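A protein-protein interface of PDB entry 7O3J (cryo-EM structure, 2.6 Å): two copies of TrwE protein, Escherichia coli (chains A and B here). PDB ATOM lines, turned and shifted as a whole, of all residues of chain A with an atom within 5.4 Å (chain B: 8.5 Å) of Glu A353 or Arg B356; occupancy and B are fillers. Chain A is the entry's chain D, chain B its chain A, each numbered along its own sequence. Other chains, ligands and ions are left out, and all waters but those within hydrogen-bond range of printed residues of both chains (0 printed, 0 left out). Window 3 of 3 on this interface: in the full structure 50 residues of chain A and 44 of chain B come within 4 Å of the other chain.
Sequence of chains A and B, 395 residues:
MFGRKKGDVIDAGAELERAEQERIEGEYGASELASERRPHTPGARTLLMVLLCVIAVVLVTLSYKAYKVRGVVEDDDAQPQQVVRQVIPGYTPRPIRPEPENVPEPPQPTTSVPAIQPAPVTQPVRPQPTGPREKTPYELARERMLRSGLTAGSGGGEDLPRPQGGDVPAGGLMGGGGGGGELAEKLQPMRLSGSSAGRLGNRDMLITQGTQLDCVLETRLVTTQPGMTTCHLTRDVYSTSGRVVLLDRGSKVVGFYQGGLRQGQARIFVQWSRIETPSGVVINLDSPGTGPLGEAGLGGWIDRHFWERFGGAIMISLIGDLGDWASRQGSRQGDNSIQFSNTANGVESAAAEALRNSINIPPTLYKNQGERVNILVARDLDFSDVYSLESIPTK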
ATOM      1  N   SER A 349      11.057   2.124   5.145  1.00  0.00           N
ATOM      2  CA  SER A 349      11.417   1.511   3.874  1.00  0.00           C
ATOM      3  C   SER A 349      12.818   1.919   3.439  1.00  0.00           C
ATOM      4  O   SER A 349      13.192   3.090   3.514  1.00  0.00           O
ATOM      5  CB  SER A 349      10.404   1.883   2.794  1.00  0.00           C
ATOM      6  OG  SER A 349      10.613   1.125   1.617  1.00  0.00           O
ATOM      7  N   ALA A 350      13.591   0.936   2.981  1.00  0.00           N
ATOM      8  CA  ALA A 350      14.946   1.208   2.522  1.00  0.00           C
ATOM      9  C   ALA A 350      14.953   2.108   1.295  1.00  0.00           C
ATOM     10  O   ALA A 350      15.813   2.984   1.174  1.00  0.00           O
ATOM     11  CB  ALA A 350      15.675  -0.100   2.227  1.00  0.00           C
ATOM     12  N   ALA A 351      14.015   1.904   0.370  1.00  0.00           N
ATOM     13  CA  ALA A 351      13.953   2.753  -0.812  1.00  0.00           C
ATOM     14  C   ALA A 351      13.648   4.196  -0.437  1.00  0.00           C
ATOM     15  O   ALA A 351      14.244   5.124  -0.991  1.00  0.00           O
ATOM     16  CB  ALA A 351      12.910   2.220  -1.789  1.00  0.00           C
ATOM     17  N   ALA A 352      12.727   4.403   0.501  1.00  0.00           N
ATOM     18  CA  ALA A 352      12.442   5.755   0.961  1.00  0.00           C
ATOM     19  C   ALA A 352      13.639   6.371   1.668  1.00  0.00           C
ATOM     20  O   ALA A 352      13.908   7.560   1.491  1.00  0.00           O
ATOM     21  CB  ALA A 352      11.226   5.756   1.879  1.00  0.00           C
ATOM     22  N   GLU A 353      14.362   5.590   2.474  1.00  0.00           N
ATOM     23  CA  GLU A 353      15.566   6.123   3.111  1.00  0.00           C
ATOM     24  C   GLU A 353      16.612   6.518   2.081  1.00  0.00           C
ATOM     25  O   GLU A 353      17.269   7.553   2.224  1.00  0.00           O
ATOM     26  CB  GLU A 353      16.153   5.106   4.085  1.00  0.00           C
ATOM     27  CG  GLU A 353      15.282   4.818   5.281  1.00  0.00           C
ATOM     28  CD  GLU A 353      15.141   6.017   6.193  1.00  0.00           C
ATOM     29  OE1 GLU A 353      16.097   6.814   6.279  1.00  0.00           O
ATOM     30  OE2 GLU A 353      14.073   6.164   6.824  1.00  0.00           O
ATOM     31  N   ALA A 354      16.800   5.696   1.051  1.00  0.00           N
ATOM     32  CA  ALA A 354      17.772   6.023   0.017  1.00  0.00           C
ATOM     33  C   ALA A 354      17.365   7.274  -0.740  1.00  0.00           C
ATOM     34  O   ALA A 354      18.206   8.121  -1.054  1.00  0.00           O
ATOM     35  CB  ALA A 354      17.935   4.849  -0.942  1.00  0.00           C
ATOM     36  N   LEU A 355      16.077   7.409  -1.045  1.00  0.00           N
ATOM     37  CA  LEU A 355      15.614   8.561  -1.805  1.00  0.00           C
ATOM     38  C   LEU A 355      15.683   9.843  -0.990  1.00  0.00           C
ATOM     39  O   LEU A 355      16.017  10.900  -1.532  1.00  0.00           O
ATOM     40  CB  LEU A 355      14.192   8.312  -2.288  1.00  0.00           C
ATOM     41  CG  LEU A 355      13.681   9.192  -3.412  1.00  0.00           C
ATOM     42  CD1 LEU A 355      14.566   9.024  -4.611  1.00  0.00           C
ATOM     43  CD2 LEU A 355      12.280   8.782  -3.742  1.00  0.00           C
ATOM     44  N   ARG A 356      15.378   9.769   0.303  1.00  0.00           N
ATOM     45  CA  ARG A 356      15.353  10.962   1.138  1.00  0.00           C
ATOM     46  C   ARG A 356      16.721  11.625   1.214  1.00  0.00           C
ATOM     47  O   ARG A 356      16.817  12.845   1.370  1.00  0.00           O
ATOM     48  CB  ARG A 356      14.859  10.596   2.533  1.00  0.00           C
ATOM     49  CG  ARG A 356      14.656  11.764   3.461  1.00  0.00           C
ATOM     50  CD  ARG A 356      14.050  11.302   4.768  1.00  0.00           C
ATOM     51  NE  ARG A 356      12.805  10.572   4.556  1.00  0.00           N
ATOM     52  CZ  ARG A 356      12.633   9.288   4.845  1.00  0.00           C
ATOM     53  NH1 ARG A 356      13.628   8.588   5.367  1.00  0.00           N
ATOM     54  NH2 ARG A 356      11.466   8.705   4.616  1.00  0.00           N
ATOM     55  N   ASN A 357      17.789  10.840   1.107  1.00  0.00           N
ATOM     56  CA  ASN A 357      19.124  11.391   1.295  1.00  0.00           C
ATOM     57  C   ASN A 357      19.690  11.974   0.007  1.00  0.00           C
ATOM     58  O   ASN A 357      20.419  12.967   0.047  1.00  0.00           O
ATOM     59  CB  ASN A 357      20.052  10.316   1.849  1.00  0.00           C
ATOM     60  CG  ASN A 357      19.700   9.926   3.268  1.00  0.00           C
ATOM     61  OD1 ASN A 357      20.188  10.523   4.225  1.00  0.00           O
ATOM     62  ND2 ASN A 357      18.848   8.923   3.413  1.00  0.00           N
ATOM     63  N   ARG B 309      28.228   2.099   0.162  1.00  0.00           N
ATOM     64  CA  ARG B 309      26.995   2.767   0.542  1.00  0.00           C
ATOM     65  C   ARG B 309      25.787   1.846   0.511  1.00  0.00           C
ATOM     66  O   ARG B 309      24.868   2.022   1.316  1.00  0.00           O
ATOM     67  CB  ARG B 309      26.744   3.962  -0.374  1.00  0.00           C
ATOM     68  CG  ARG B 309      27.719   5.089  -0.180  1.00  0.00           C
ATOM     69  CD  ARG B 309      27.216   6.361  -0.797  1.00  0.00           C
ATOM     70  NE  ARG B 309      27.022   6.233  -2.230  1.00  0.00           N
ATOM     71  CZ  ARG B 309      26.027   6.800  -2.897  1.00  0.00           C
ATOM     72  NH1 ARG B 309      25.133   7.531  -2.254  1.00  0.00           N
ATOM     73  NH2 ARG B 309      25.929   6.633  -4.204  1.00  0.00           N
ATOM     74  N   PHE B 310      25.757   0.866  -0.392  1.00  0.00           N
ATOM     75  CA  PHE B 310      24.578   0.032  -0.554  1.00  0.00           C
ATOM     76  C   PHE B 310      24.794  -1.446  -0.277  1.00  0.00           C
ATOM     77  O   PHE B 310      23.808  -2.188  -0.230  1.00  0.00           O
ATOM     78  CB  PHE B 310      24.013   0.179  -1.973  1.00  0.00           C
ATOM     79  CG  PHE B 310      23.539   1.557  -2.290  1.00  0.00           C
ATOM     80  CD1 PHE B 310      22.331   2.010  -1.812  1.00  0.00           C
ATOM     81  CD2 PHE B 310      24.302   2.403  -3.064  1.00  0.00           C
ATOM     82  CE1 PHE B 310      21.897   3.278  -2.101  1.00  0.00           C
ATOM     83  CE2 PHE B 310      23.869   3.669  -3.354  1.00  0.00           C
ATOM     84  CZ  PHE B 310      22.668   4.107  -2.871  1.00  0.00           C
ATOM     85  N   ALA B 313      23.033  -2.840   2.968  1.00  0.00           N
ATOM     86  CA  ALA B 313      21.594  -3.006   2.799  1.00  0.00           C
ATOM     87  C   ALA B 313      21.270  -4.162   1.864  1.00  0.00           C
ATOM     88  O   ALA B 313      20.372  -4.962   2.148  1.00  0.00           O
ATOM     89  CB  ALA B 313      20.978  -1.710   2.280  1.00  0.00           C
ATOM     90  N   SER B 349      13.451  -1.903  10.300  1.00  0.00           N
ATOM     91  CA  SER B 349      14.066  -2.819   9.351  1.00  0.00           C
ATOM     92  C   SER B 349      15.586  -2.736   9.407  1.00  0.00           C
ATOM     93  O   SER B 349      16.164  -1.648   9.447  1.00  0.00           O
ATOM     94  CB  SER B 349      13.578  -2.528   7.933  1.00  0.00           C
ATOM     95  OG  SER B 349      13.994  -3.540   7.035  1.00  0.00           O
ATOM     96  N   ALA B 350      16.230  -3.903   9.407  1.00  0.00           N
ATOM     97  CA  ALA B 350      17.685  -3.948   9.445  1.00  0.00           C
ATOM     98  C   ALA B 350      18.297  -3.339   8.191  1.00  0.00           C
ATOM     99  O   ALA B 350      19.320  -2.656   8.271  1.00  0.00           O
ATOM    100  CB  ALA B 350      18.161  -5.388   9.625  1.00  0.00           C
ATOM    101  N   ALA B 351      17.698  -3.585   7.025  1.00  0.00           N
ATOM    102  CA  ALA B 351      18.222  -3.005   5.796  1.00  0.00           C
ATOM    103  C   ALA B 351      18.138  -1.487   5.826  1.00  0.00           C
ATOM    104  O   ALA B 351      19.074  -0.800   5.404  1.00  0.00           O
ATOM    105  CB  ALA B 351      17.472  -3.562   4.590  1.00  0.00           C
ATOM    106  N   ALA B 352      17.027  -0.944   6.321  1.00  0.00           N
ATOM    107  CA  ALA B 352      16.913   0.501   6.448  1.00  0.00           C
ATOM    108  C   ALA B 352      17.911   1.058   7.450  1.00  0.00           C
ATOM    109  O   ALA B 352      18.482   2.126   7.219  1.00  0.00           O
ATOM    110  CB  ALA B 352      15.493   0.887   6.847  1.00  0.00           C
ATOM    111  N   GLU B 353      18.136   0.362   8.567  1.00  0.00           N
ATOM    112  CA  GLU B 353      19.146   0.820   9.518  1.00  0.00           C
ATOM    113  C   GLU B 353      20.535   0.820   8.900  1.00  0.00           C
ATOM    114  O   GLU B 353      21.319   1.746   9.125  1.00  0.00           O
ATOM    115  CB  GLU B 353      19.135  -0.048  10.773  1.00  0.00           C
ATOM    116  CG  GLU B 353      17.876   0.063  11.594  1.00  0.00           C
ATOM    117  CD  GLU B 353      17.710   1.433  12.213  1.00  0.00           C
ATOM    118  OE1 GLU B 353      18.736   2.072  12.529  1.00  0.00           O
ATOM    119  OE2 GLU B 353      16.555   1.876  12.381  1.00  0.00           O
ATOM    120  N   ALA B 354      20.866  -0.219   8.138  1.00  0.00           N
ATOM    121  CA  ALA B 354      22.173  -0.273   7.497  1.00  0.00           C
ATOM    122  C   ALA B 354      22.327   0.839   6.475  1.00  0.00           C
ATOM    123  O   ALA B 354      23.390   1.457   6.374  1.00  0.00           O
ATOM    124  CB  ALA B 354      22.381  -1.635   6.840  1.00  0.00           C
ATOM    125  N   LEU B 355      21.277   1.105   5.703  1.00  0.00           N
ATOM    126  CA  LEU B 355      21.361   2.129   4.673  1.00  0.00           C
ATOM    127  C   LEU B 355      21.437   3.526   5.265  1.00  0.00           C
ATOM    128  O   LEU B 355      22.157   4.381   4.742  1.00  0.00           O
ATOM    129  CB  LEU B 355      20.162   2.012   3.741  1.00  0.00           C
ATOM    130  CG  LEU B 355      20.260   2.704   2.396  1.00  0.00           C
ATOM    131  CD1 LEU B 355      21.432   2.149   1.643  1.00  0.00           C
ATOM    132  CD2 LEU B 355      18.994   2.456   1.636  1.00  0.00           C
ATOM    133  N   ARG B 356      20.713   3.776   6.354  1.00  0.00           N
ATOM    134  CA  ARG B 356      20.677   5.108   6.943  1.00  0.00           C
ATOM    135  C   ARG B 356      22.052   5.548   7.420  1.00  0.00           C
ATOM    136  O   ARG B 356      22.359   6.744   7.428  1.00  0.00           O
ATOM    137  CB  ARG B 356      19.680   5.125   8.096  1.00  0.00           C
ATOM    138  CG  ARG B 356      19.445   6.480   8.711  1.00  0.00           C
ATOM    139  CD  ARG B 356      18.352   6.404   9.756  1.00  0.00           C
ATOM    140  NE  ARG B 356      17.121   5.850   9.206  1.00  0.00           N
ATOM    141  CZ  ARG B 356      16.581   4.699   9.593  1.00  0.00           C
ATOM    142  NH1 ARG B 356      17.166   3.977  10.535  1.00  0.00           N
ATOM    143  NH2 ARG B 356      15.459   4.272   9.035  1.00  0.00           N
ATOM    144  N   ASN B 357      22.894   4.601   7.825  1.00  0.00           N
ATOM    145  CA  ASN B 357      24.177   4.963   8.409  1.00  0.00           C
ATOM    146  C   ASN B 357      25.252   5.166   7.351  1.00  0.00           C
ATOM    147  O   ASN B 357      26.129   6.018   7.515  1.00  0.00           O
ATOM    148  CB  ASN B 357      24.608   3.896   9.410  1.00  0.00           C
ATOM    149  CG  ASN B 357      23.729   3.874  10.642  1.00  0.00           C
ATOM    150  OD1 ASN B 357      23.989   4.576  11.617  1.00  0.00           O
ATOM    151  ND2 ASN B 357      22.676   3.071  10.604  1.00  0.00           N
ATOM    152  N   SER B 358      25.206   4.403   6.264  1.00  0.00           N
ATOM    153  CA  SER B 358      26.262   4.427   5.264  1.00  0.00           C
ATOM    154  C   SER B 358      25.841   5.071   3.953  1.00  0.00           C
ATOM    155  O   SER B 358      26.612   5.042   2.992  1.00  0.00           O
ATOM    156  CB  SER B 358      26.759   3.009   5.008  1.00  0.00           C
ATOM    157  OG  SER B 358      25.677   2.105   4.917  1.00  0.00           O
ATOM    158  N   ILE B 359      24.648   5.657   3.885  1.00  0.00           N
ATOM    159  CA  ILE B 359      24.208   6.255   2.631  1.00  0.00           C
ATOM    160  C   ILE B 359      24.986   7.527   2.318  1.00  0.00           C
ATOM    161  O   ILE B 359      25.200   7.855   1.147  1.00  0.00           O
ATOM    162  CB  ILE B 359      22.688   6.500   2.673  1.00  0.00           C
ATOM    163  CG1 ILE B 359      22.155   6.829   1.285  1.00  0.00           C
ATOM    164  CG2 ILE B 359      22.341   7.597   3.655  1.00  0.00           C
ATOM    165  CD1 ILE B 359      22.383   5.745   0.294  1.00  0.00           C
ATOM    166  N   ASN B 360      25.422   8.265   3.337  1.00  0.00           N
ATOM    167  CA  ASN B 360      26.061   9.564   3.137  1.00  0.00           C
ATOM    168  C   ASN B 360      27.575   9.413   3.237  1.00  0.00           C
ATOM    169  O   ASN B 360      28.197   9.734   4.246  1.00  0.00           O
ATOM    170  CB  ASN B 360      25.538  10.576   4.143  1.00  0.00           C
ATOM    171  CG  ASN B 360      24.061  10.826   3.996  1.00  0.00           C
ATOM    172  OD1 ASN B 360      23.586  11.180   2.921  1.00  0.00           O
ATOM    173  ND2 ASN B 360      23.322  10.652   5.082  1.00  0.00           N
ATOM    174  N   ILE B 361      28.172   8.920   2.159  1.00  0.00           N
ATOM    175  CA  ILE B 361      29.622   8.853   2.036  1.00  0.00           C
ATOM    176  C   ILE B 361      30.017   9.737   0.862  1.00  0.00           C
ATOM    177  O   ILE B 361      29.611   9.464  -0.274  1.00  0.00           O
ATOM    178  CB  ILE B 361      30.103   7.408   1.847  1.00  0.00           C
ATOM    179  CG1 ILE B 361      29.910   6.615   3.135  1.00  0.00           C
ATOM    180  CG2 ILE B 361      31.548   7.377   1.438  1.00  0.00           C
ATOM    181  CD1 ILE B 361      30.340   5.186   3.024  1.00  0.00           C
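Ala A350 touches Leu B355, but with the chains exchanged Leu A355 does not touch Ala B350 (14.1 Å). Glu A353 touches Arg B356, but with the chains exchanged Arg A356 does not touch Glu B353 (9.9 Å). Ala A354 touches Leu B355, but with the chains exchanged Leu A355 does not touch Ala B354 (11.8 Å). Positions printed for both chains: 349, 350, 351, 352, 353, 354, 355, 356 and 357.
NH2 of Arg B356 is in salt-bridge range of OE2 of Glu A353 (3.2 Å). OD1 of Asn A357 is in hydrogen-bond range of ND2 of Asn B360 (3.3 Å).
Of the printed residues of chain B, Glu A353 touches Arg B356. No residue of chain B comes within 4 Å of Ala A352. Of chain B, only Leu B355 (3.7 Å) comes within 4 Å of Ala A354. Printed residues of chain A within 4 Å of Ile B359: Asn A357. Of the printed residues of chain A, Leu B355 touches Ala A350 and Ala A354. Leu A355 touches none of the printed residues of chain B. The nearest printed residue of chain A that does not touch Arg B356 is Asn A357 (5.4 Å). The nearest printed residue of chain A that does not touch Asn B360 is Arg A356 (7.1 Å).
Hydrophobic or aromatic side chains of chain A within 4 Å of the printed part of chain B: Ala A354. Among the printed residues, 5 pairs touch across the chains.
NH1 of Arg B309 lies close to O of Ile B359, 3.4 Å away. The side-chain carboxylate of Glu B353 lies within salt-bridge range of the guanidinium group of Arg B356 (2.9 Å). The side-chain carboxylate of Glu A353 lies within salt-bridge range of the guanidinium group of Arg A356, 2.9 Å away. ND2 of Asn A357 lies within hydrogen-bond range of O of Glu A353, 2.4 Å away.
Ala A350 touches Leu B355 (O to CD2, 3.3 Å). Leu B355 touches Ala A354 (CD2 to CB, 3.7 Å). Asn A357 touches Ile B359.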
